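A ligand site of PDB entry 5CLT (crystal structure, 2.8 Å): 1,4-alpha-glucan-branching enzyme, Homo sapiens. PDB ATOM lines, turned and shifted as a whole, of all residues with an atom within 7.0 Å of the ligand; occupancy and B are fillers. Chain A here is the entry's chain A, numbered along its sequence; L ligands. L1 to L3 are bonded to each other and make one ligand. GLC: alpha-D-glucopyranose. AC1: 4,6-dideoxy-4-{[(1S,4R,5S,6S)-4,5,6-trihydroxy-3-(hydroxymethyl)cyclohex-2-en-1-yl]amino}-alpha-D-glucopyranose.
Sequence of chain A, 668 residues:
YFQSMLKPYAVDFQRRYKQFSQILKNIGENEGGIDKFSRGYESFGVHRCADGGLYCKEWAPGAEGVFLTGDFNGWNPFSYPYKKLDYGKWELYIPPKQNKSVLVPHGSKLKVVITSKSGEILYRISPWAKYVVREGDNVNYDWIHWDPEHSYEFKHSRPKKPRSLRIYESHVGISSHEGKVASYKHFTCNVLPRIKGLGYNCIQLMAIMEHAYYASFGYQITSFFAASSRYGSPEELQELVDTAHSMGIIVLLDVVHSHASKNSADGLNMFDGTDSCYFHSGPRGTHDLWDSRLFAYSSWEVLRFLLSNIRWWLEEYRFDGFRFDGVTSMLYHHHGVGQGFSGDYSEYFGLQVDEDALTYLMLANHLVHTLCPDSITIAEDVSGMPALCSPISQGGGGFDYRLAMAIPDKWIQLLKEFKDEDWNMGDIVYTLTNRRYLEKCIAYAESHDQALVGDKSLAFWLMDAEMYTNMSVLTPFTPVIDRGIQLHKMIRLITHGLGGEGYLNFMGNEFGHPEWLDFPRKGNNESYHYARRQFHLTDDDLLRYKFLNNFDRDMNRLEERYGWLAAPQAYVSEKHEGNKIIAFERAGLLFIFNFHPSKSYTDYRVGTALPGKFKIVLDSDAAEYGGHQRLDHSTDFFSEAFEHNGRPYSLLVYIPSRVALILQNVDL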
ATOM      1  N   ASN A  26      27.046  -1.311 -37.781  1.00  0.00           N
ATOM      2  CA  ASN A  26      26.380  -1.412 -36.502  1.00  0.00           C
ATOM      3  C   ASN A  26      26.389  -2.844 -35.988  1.00  0.00           C
ATOM      4  O   ASN A  26      26.589  -3.083 -34.801  1.00  0.00           O
ATOM      5  CB  ASN A  26      24.926  -0.928 -36.574  1.00  0.00           C
ATOM      6  CG  ASN A  26      24.819   0.536 -36.837  1.00  0.00           C
ATOM      7  OD1 ASN A  26      25.780   1.292 -36.602  1.00  0.00           O
ATOM      8  ND2 ASN A  26      23.679   0.960 -37.354  1.00  0.00           N
ATOM      9  N   GLU A  29      29.641  -3.177 -34.461  1.00  0.00           N
ATOM     10  CA  GLU A  29      29.926  -2.458 -33.232  1.00  0.00           C
ATOM     11  C   GLU A  29      29.003  -2.936 -32.088  1.00  0.00           C
ATOM     12  O   GLU A  29      29.367  -2.859 -30.924  1.00  0.00           O
ATOM     13  CB  GLU A  29      29.810  -0.953 -33.466  1.00  0.00           C
ATOM     14  N   ASN A  30      27.825  -3.460 -32.427  1.00  0.00           N
ATOM     15  CA  ASN A  30      26.828  -3.895 -31.442  1.00  0.00           C
ATOM     16  C   ASN A  30      26.644  -5.373 -31.210  1.00  0.00           C
ATOM     17  O   ASN A  30      26.128  -5.772 -30.162  1.00  0.00           O
ATOM     18  CB  ASN A  30      25.483  -3.318 -31.811  1.00  0.00           C
ATOM     19  CG  ASN A  30      25.427  -1.827 -31.591  1.00  0.00           C
ATOM     20  OD1 ASN A  30      26.224  -1.281 -30.832  1.00  0.00           O
ATOM     21  ND2 ASN A  30      24.521  -1.164 -32.293  1.00  0.00           N
ATOM     22  N   GLU A  31      26.984  -6.181 -32.213  1.00  0.00           N
ATOM     23  CA  GLU A  31      26.840  -7.642 -32.141  1.00  0.00           C
ATOM     24  C   GLU A  31      28.165  -8.381 -32.431  1.00  0.00           C
ATOM     25  O   GLU A  31      28.213  -9.590 -32.487  1.00  0.00           O
ATOM     26  CB  GLU A  31      25.742  -8.115 -33.103  1.00  0.00           C
ATOM     27  CG  GLU A  31      24.345  -7.489 -32.903  1.00  0.00           C
ATOM     28  CD  GLU A  31      23.570  -8.111 -31.741  1.00  0.00           C
ATOM     29  OE1 GLU A  31      23.967  -9.205 -31.236  1.00  0.00           O
ATOM     30  OE2 GLU A  31      22.579  -7.499 -31.303  1.00  0.00           O
ATOM     31  N   PHE A  37      26.619 -12.435 -35.086  1.00  0.00           N
ATOM     32  CA  PHE A  37      25.226 -12.029 -35.145  1.00  0.00           C
ATOM     33  C   PHE A  37      24.335 -13.160 -35.617  1.00  0.00           C
ATOM     34  O   PHE A  37      23.261 -13.380 -35.051  1.00  0.00           O
ATOM     35  CB  PHE A  37      25.060 -10.798 -36.054  1.00  0.00           C
ATOM     36  CG  PHE A  37      23.681 -10.185 -35.997  1.00  0.00           C
ATOM     37  CD1 PHE A  37      23.015 -10.021 -34.787  1.00  0.00           C
ATOM     38  CD2 PHE A  37      23.080  -9.689 -37.152  1.00  0.00           C
ATOM     39  CE1 PHE A  37      21.763  -9.424 -34.741  1.00  0.00           C
ATOM     40  CE2 PHE A  37      21.834  -9.093 -37.099  1.00  0.00           C
ATOM     41  CZ  PHE A  37      21.175  -8.962 -35.914  1.00  0.00           C
ATOM     42  N   TRP A  59      12.302 -13.849 -27.791  1.00  0.00           N
ATOM     43  CA  TRP A  59      12.054 -12.442 -27.985  1.00  0.00           C
ATOM     44  C   TRP A  59      10.558 -12.288 -28.029  1.00  0.00           C
ATOM     45  O   TRP A  59       9.909 -12.854 -28.890  1.00  0.00           O
ATOM     46  CB  TRP A  59      12.684 -11.953 -29.253  1.00  0.00           C
ATOM     47  CG  TRP A  59      12.505 -10.519 -29.467  1.00  0.00           C
ATOM     48  CD1 TRP A  59      12.908  -9.526 -28.625  1.00  0.00           C
ATOM     49  CD2 TRP A  59      11.937  -9.871 -30.615  1.00  0.00           C
ATOM     50  NE1 TRP A  59      12.603  -8.303 -29.169  1.00  0.00           N
ATOM     51  CE2 TRP A  59      12.008  -8.482 -30.380  1.00  0.00           C
ATOM     52  CE3 TRP A  59      11.374 -10.325 -31.803  1.00  0.00           C
ATOM     53  CZ2 TRP A  59      11.543  -7.552 -31.304  1.00  0.00           C
ATOM     54  CZ3 TRP A  59      10.897  -9.390 -32.700  1.00  0.00           C
ATOM     55  CH2 TRP A  59      10.988  -8.020 -32.460  1.00  0.00           C
ATOM     56  N   ALA A  60      10.007 -11.536 -27.098  1.00  0.00           N
ATOM     57  CA  ALA A  60       8.565 -11.414 -26.976  1.00  0.00           C
ATOM     58  C   ALA A  60       8.266 -10.119 -26.294  1.00  0.00           C
ATOM     59  O   ALA A  60       7.894 -10.108 -25.123  1.00  0.00           O
ATOM     60  CB  ALA A  60       7.991 -12.567 -26.199  1.00  0.00           C
ATOM     61  N   PRO A  61       8.411  -9.001 -27.031  1.00  0.00           N
ATOM     62  CA  PRO A  61       8.344  -7.671 -26.425  1.00  0.00           C
ATOM     63  C   PRO A  61       6.959  -7.282 -25.926  1.00  0.00           C
ATOM     64  O   PRO A  61       6.853  -6.456 -25.031  1.00  0.00           O
ATOM     65  CB  PRO A  61       8.835  -6.761 -27.550  1.00  0.00           C
ATOM     66  CG  PRO A  61       8.656  -7.522 -28.803  1.00  0.00           C
ATOM     67  CD  PRO A  61       8.714  -8.955 -28.474  1.00  0.00           C
ATOM     68  N   GLY A  62       5.924  -7.901 -26.431  1.00  0.00           N
ATOM     69  CA  GLY A  62       4.586  -7.576 -25.958  1.00  0.00           C
ATOM     70  C   GLY A  62       4.042  -8.538 -24.931  1.00  0.00           C
ATOM     71  O   GLY A  62       2.863  -8.498 -24.571  1.00  0.00           O
ATOM     72  N   ALA A  63       4.878  -9.431 -24.435  1.00  0.00           N
ATOM     73  CA  ALA A  63       4.354 -10.379 -23.465  1.00  0.00           C
ATOM     74  C   ALA A  63       4.356  -9.758 -22.081  1.00  0.00           C
ATOM     75  O   ALA A  63       5.246  -8.985 -21.748  1.00  0.00           O
ATOM     76  CB  ALA A  63       5.171 -11.678 -23.459  1.00  0.00           C
ATOM     77  N   LEU A  85      14.208  -9.625 -19.561  1.00  0.00           N
ATOM     78  CA  LEU A  85      15.479  -8.959 -19.828  1.00  0.00           C
ATOM     79  C   LEU A  85      15.317  -7.636 -20.546  1.00  0.00           C
ATOM     80  O   LEU A  85      14.221  -7.239 -20.887  1.00  0.00           O
ATOM     81  CB  LEU A  85      16.374  -9.894 -20.655  1.00  0.00           C
ATOM     82  CG  LEU A  85      16.875 -11.071 -19.804  1.00  0.00           C
ATOM     83  CD1 LEU A  85      17.847 -11.932 -20.555  1.00  0.00           C
ATOM     84  CD2 LEU A  85      17.493 -10.544 -18.532  1.00  0.00           C
ATOM     85  N   ASP A  86      16.409  -6.925 -20.760  1.00  0.00           N
ATOM     86  CA  ASP A  86      16.335  -5.716 -21.580  1.00  0.00           C
ATOM     87  C   ASP A  86      15.873  -6.057 -22.998  1.00  0.00           C
ATOM     88  O   ASP A  86      15.934  -7.212 -23.418  1.00  0.00           O
ATOM     89  CB  ASP A  86      17.704  -5.015 -21.615  1.00  0.00           C
ATOM     90  CG  ASP A  86      17.983  -4.197 -20.350  1.00  0.00           C
ATOM     91  OD1 ASP A  86      17.060  -4.020 -19.518  1.00  0.00           O
ATOM     92  OD2 ASP A  86      19.134  -3.710 -20.212  1.00  0.00           O
ATOM     93  N   TYR A  87      15.395  -5.053 -23.732  1.00  0.00           N
ATOM     94  CA  TYR A  87      15.096  -5.243 -25.155  1.00  0.00           C
ATOM     95  C   TYR A  87      14.041  -6.326 -25.478  1.00  0.00           C
ATOM     96  O   TYR A  87      14.113  -6.985 -26.509  1.00  0.00           O
ATOM     97  CB  TYR A  87      16.379  -5.580 -25.896  1.00  0.00           C
ATOM     98  CG  TYR A  87      17.485  -4.554 -25.699  1.00  0.00           C
ATOM     99  CD1 TYR A  87      17.306  -3.227 -26.097  1.00  0.00           C
ATOM    100  CD2 TYR A  87      18.693  -4.910 -25.125  1.00  0.00           C
ATOM    101  CE1 TYR A  87      18.301  -2.286 -25.934  1.00  0.00           C
ATOM    102  CE2 TYR A  87      19.698  -3.979 -24.959  1.00  0.00           C
ATOM    103  CZ  TYR A  87      19.496  -2.669 -25.364  1.00  0.00           C
ATOM    104  OH  TYR A  87      20.498  -1.723 -25.207  1.00  0.00           O
ATOM    105  N   GLY A  88      13.057  -6.488 -24.614  1.00  0.00           N
ATOM    106  CA  GLY A  88      11.985  -7.412 -24.910  1.00  0.00           C
ATOM    107  C   GLY A  88      12.377  -8.880 -24.903  1.00  0.00           C
ATOM    108  O   GLY A  88      11.580  -9.742 -25.269  1.00  0.00           O
ATOM    109  N   LYS A  89      13.578  -9.200 -24.468  1.00  0.00           N
ATOM    110  CA  LYS A  89      13.935 -10.612 -24.502  1.00  0.00           C
ATOM    111  C   LYS A  89      13.637 -11.255 -23.171  1.00  0.00           C
ATOM    112  O   LYS A  89      13.398 -10.579 -22.160  1.00  0.00           O
ATOM    113  CB  LYS A  89      15.401 -10.802 -24.908  1.00  0.00           C
ATOM    114  CG  LYS A  89      15.724 -10.058 -26.163  1.00  0.00           C
ATOM    115  CD  LYS A  89      17.065 -10.400 -26.668  1.00  0.00           C
ATOM    116  CE  LYS A  89      17.514  -9.464 -27.762  1.00  0.00           C
ATOM    117  NZ  LYS A  89      18.682  -8.635 -27.351  1.00  0.00           N
ATOM    118  N   TRP A  90      13.587 -12.576 -23.180  1.00  0.00           N
ATOM    119  CA  TRP A  90      13.290 -13.352 -21.983  1.00  0.00           C
ATOM    120  C   TRP A  90      14.208 -14.554 -21.905  1.00  0.00           C
ATOM    121  O   TRP A  90      14.433 -15.212 -22.915  1.00  0.00           O
ATOM    122  CB  TRP A  90      11.842 -13.812 -21.988  1.00  0.00           C
ATOM    123  CG  TRP A  90      10.829 -12.706 -21.977  1.00  0.00           C
ATOM    124  CD1 TRP A  90      10.473 -11.918 -23.026  1.00  0.00           C
ATOM    125  CD2 TRP A  90      10.011 -12.301 -20.862  1.00  0.00           C
ATOM    126  NE1 TRP A  90       9.489 -11.049 -22.638  1.00  0.00           N
ATOM    127  CE2 TRP A  90       9.188 -11.256 -21.319  1.00  0.00           C
ATOM    128  CE3 TRP A  90       9.901 -12.712 -19.534  1.00  0.00           C
ATOM    129  CZ2 TRP A  90       8.282 -10.632 -20.501  1.00  0.00           C
ATOM    130  CZ3 TRP A  90       9.005 -12.091 -18.727  1.00  0.00           C
ATOM    131  CH2 TRP A  90       8.199 -11.059 -19.215  1.00  0.00           C
ATOM    132  N   SER A 299      13.463  -4.413 -38.375  1.00  0.00           N
ATOM    133  CA  SER A 299      13.578  -4.712 -36.979  1.00  0.00           C
ATOM    134  C   SER A 299      14.797  -5.605 -36.652  1.00  0.00           C
ATOM    135  O   SER A 299      14.967  -6.693 -37.207  1.00  0.00           O
ATOM    136  CB  SER A 299      12.275  -5.349 -36.498  1.00  0.00           C
ATOM    137  OG  SER A 299      12.461  -5.929 -35.242  1.00  0.00           O
ATOM    138  N   TRP A 300      15.653  -5.109 -35.776  1.00  0.00           N
ATOM    139  CA  TRP A 300      16.908  -5.775 -35.420  1.00  0.00           C
ATOM    140  C   TRP A 300      16.747  -7.261 -35.018  1.00  0.00           C
ATOM    141  O   TRP A 300      17.601  -8.075 -35.358  1.00  0.00           O
ATOM    142  CB  TRP A 300      17.568  -5.012 -34.289  1.00  0.00           C
ATOM    143  CG  TRP A 300      19.011  -5.294 -34.064  1.00  0.00           C
ATOM    144  CD1 TRP A 300      19.549  -6.094 -33.106  1.00  0.00           C
ATOM    145  CD2 TRP A 300      20.113  -4.720 -34.780  1.00  0.00           C
ATOM    146  NE1 TRP A 300      20.911  -6.078 -33.186  1.00  0.00           N
ATOM    147  CE2 TRP A 300      21.295  -5.253 -34.209  1.00  0.00           C
ATOM    148  CE3 TRP A 300      20.226  -3.842 -35.856  1.00  0.00           C
ATOM    149  CZ2 TRP A 300      22.560  -4.927 -34.676  1.00  0.00           C
ATOM    150  CZ3 TRP A 300      21.504  -3.511 -36.321  1.00  0.00           C
ATOM    151  CH2 TRP A 300      22.650  -4.056 -35.731  1.00  0.00           C
ATOM    152  N   GLU A 301      15.688  -7.612 -34.306  1.00  0.00           N
ATOM    153  CA  GLU A 301      15.530  -9.012 -33.907  1.00  0.00           C
ATOM    154  C   GLU A 301      15.039  -9.827 -35.108  1.00  0.00           C
ATOM    155  O   GLU A 301      15.307 -11.025 -35.204  1.00  0.00           O
ATOM    156  CB  GLU A 301      14.562  -9.158 -32.723  1.00  0.00           C
ATOM    157  CG  GLU A 301      15.085  -8.634 -31.402  1.00  0.00           C
ATOM    158  CD  GLU A 301      16.448  -9.175 -31.087  1.00  0.00           C
ATOM    159  OE1 GLU A 301      16.668 -10.409 -31.241  1.00  0.00           O
ATOM    160  OE2 GLU A 301      17.318  -8.368 -30.744  1.00  0.00           O
ATOM    161  N   ARG A 304      18.095 -10.598 -36.764  1.00  0.00           N
ATOM    162  CA  ARG A 304      18.822 -11.672 -36.097  1.00  0.00           C
ATOM    163  C   ARG A 304      18.188 -13.018 -36.471  1.00  0.00           C
ATOM    164  O   ARG A 304      18.881 -13.949 -36.845  1.00  0.00           O
ATOM    165  CB  ARG A 304      18.873 -11.476 -34.576  1.00  0.00           C
ATOM    166  CG  ARG A 304      19.790 -12.483 -33.871  1.00  0.00           C
ATOM    167  CD  ARG A 304      19.549 -12.539 -32.363  1.00  0.00           C
ATOM    168  NE  ARG A 304      19.354 -11.218 -31.790  1.00  0.00           N
ATOM    169  CZ  ARG A 304      20.334 -10.365 -31.473  1.00  0.00           C
ATOM    170  NH1 ARG A 304      21.604 -10.673 -31.712  1.00  0.00           N
ATOM    171  NH2 ARG A 304      20.012  -9.185 -30.955  1.00  0.00           N
HETATM  172  C1  GLC L   1      11.117  -1.834 -23.125  1.00  0.00           C
HETATM  173  C2  GLC L   1      12.164  -1.165 -24.038  1.00  0.00           C
HETATM  174  C3  GLC L   1      11.944  -1.414 -25.518  1.00  0.00           C
HETATM  175  C4  GLC L   1      11.735  -2.935 -25.699  1.00  0.00           C
HETATM  176  C5  GLC L   1      10.453  -3.242 -24.895  1.00  0.00           C
HETATM  177  C6  GLC L   1       9.725  -4.564 -25.135  1.00  0.00           C
HETATM  178  O1  GLC L   1       9.909  -1.076 -23.124  1.00  0.00           O
HETATM  179  O2  GLC L   1      12.184   0.256 -23.833  1.00  0.00           O
HETATM  180  O3  GLC L   1      13.087  -0.854 -26.179  1.00  0.00           O
HETATM  181  O4  GLC L   1      11.650  -3.511 -27.025  1.00  0.00           O
HETATM  182  O5  GLC L   1      10.809  -3.191 -23.506  1.00  0.00           O
HETATM  183  O6  GLC L   1       9.161  -4.936 -23.856  1.00  0.00           O
HETATM  184  C1  GLC L   2      11.963  -2.792 -28.261  1.00  0.00           C
HETATM  185  C2  GLC L   2      12.293  -3.834 -29.306  1.00  0.00           C
HETATM  186  C3  GLC L   2      13.694  -4.399 -29.100  1.00  0.00           C
HETATM  187  C4  GLC L   2      14.687  -3.279 -29.322  1.00  0.00           C
HETATM  188  C5  GLC L   2      14.397  -2.218 -28.284  1.00  0.00           C
HETATM  189  C6  GLC L   2      15.241  -0.980 -28.569  1.00  0.00           C
HETATM  190  O2  GLC L   2      11.313  -4.879 -29.237  1.00  0.00           O
HETATM  191  O3  GLC L   2      13.940  -5.442 -30.024  1.00  0.00           O
HETATM  192  O4  GLC L   2      16.036  -3.741 -29.189  1.00  0.00           O
HETATM  193  O5  GLC L   2      13.021  -1.812 -28.263  1.00  0.00           O
HETATM  194  O6  GLC L   2      14.868  -0.421 -29.832  1.00  0.00           O
HETATM  195  C1  AC1 L   3      16.694  -3.970 -30.416  1.00  0.00           C
HETATM  196  O2  AC1 L   3      16.697  -6.258 -29.782  1.00  0.00           O
HETATM  197  C2  AC1 L   3      17.548  -5.210 -30.269  1.00  0.00           C
HETATM  198  C4A AC1 L   3      23.834  -3.452 -26.793  1.00  0.00           C
HETATM  199  C3  AC1 L   3      18.694  -4.974 -29.320  1.00  0.00           C
HETATM  200  O3  AC1 L   3      19.440  -6.188 -29.165  1.00  0.00           O
HETATM  201  C4  AC1 L   3      19.593  -3.883 -29.874  1.00  0.00           C
HETATM  202  N4A AC1 L   3      20.675  -3.661 -28.924  1.00  0.00           N
HETATM  203  C5  AC1 L   3      18.761  -2.625 -30.108  1.00  0.00           C
HETATM  204  O5  AC1 L   3      17.521  -2.865 -30.801  1.00  0.00           O
HETATM  205  C6  AC1 L   3      19.521  -1.616 -30.972  1.00  0.00           C
HETATM  206  C1B AC1 L   3      22.078  -3.623 -29.288  1.00  0.00           C
HETATM  207  C2B AC1 L   3      22.804  -4.826 -28.696  1.00  0.00           C
HETATM  208  O2B AC1 L   3      22.014  -5.989 -28.964  1.00  0.00           O
HETATM  209  C3B AC1 L   3      23.029  -4.700 -27.185  1.00  0.00           C
HETATM  210  O3B AC1 L   3      23.775  -5.836 -26.726  1.00  0.00           O
HETATM  211  O4  AC1 L   3      23.540  -3.033 -25.452  1.00  0.00           O
HETATM  212  C5B AC1 L   3      23.584  -2.297 -27.733  1.00  0.00           C
HETATM  213  C7B AC1 L   3      22.784  -2.348 -28.841  1.00  0.00           C
HETATM  214  C6B AC1 L   3      24.322  -1.029 -27.385  1.00  0.00           C
HETATM  215  O6B AC1 L   3      24.853  -0.469 -28.590  1.00  0.00           O
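The side-chain carboxylate (OE2) of Glu 301 is in salt-bridge range of the side-chain amino group (NZ) of Lys 89 (3.7 Å). OE2 of Glu 301 lies within salt-bridge range of NH2 of Arg 304, at 2.8 Å. NH1 of Arg 304 lies within salt-bridge range of OE1 of Glu 31. OE2 of Glu 31 lies within hydrogen-bond range of NE1 of Trp 300 (2.9 Å). The indole nitrogen (NE1) of Trp 59 lies within hydrogen-bond range of the backbone carbonyl oxygen (O) of Tyr 87, 3.3 Å away. O of Gly 88 lies within hydrogen-bond range of N of Ala 60.
The side-chain carboxylate of Glu 301 sits at hydrogen-bond distance from an oxygen (O2) of AC1 L3, at 2.4 Å. The side-chain amide oxygen (OD1) of Asn 30 sits at hydrogen-bond distance from an oxygen (O6B) of AC1 L3, 2.8 Å away. An oxygen (O2B) of AC1 L3 is in hydrogen-bond range of the side-chain carboxylate of Glu 31 (2.8 Å). The backbone carbonyl oxygen (O) of Pro 61 lies within hydrogen-bond range of an oxygen (O6) of GLC L1, at 3.0 Å. The side-chain amino group (NZ) of Lys 89 is in hydrogen-bond range of an oxygen (O3) of AC1 L3 (3.1 Å). An oxygen (O3) of GLC L2 is in hydrogen-bond range of the indole nitrogen (NE1) of Trp 59 (3.3 Å). The side-chain hydroxyl (OH) of Tyr 87 is in hydrogen-bond range of an oxygen (O4) of AC1 L3 (3.3 Å).
Merely in contact with the ligand: Gly 88, Trp 300 and Arg 304. Hydrophobic or aromatic side chains that line the ligand: Trp 59, Pro 61, Tyr 87 and Trp 300. Within 4 Å of the ligand: Asn 30, Glu 31, Trp 59, Pro 61, Tyr 87, Gly 88, Lys 89, Trp 300, Glu 301 and Arg 304. The nearest printed residue that does not touch the ligand is Gly 62 (5.1 Å).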
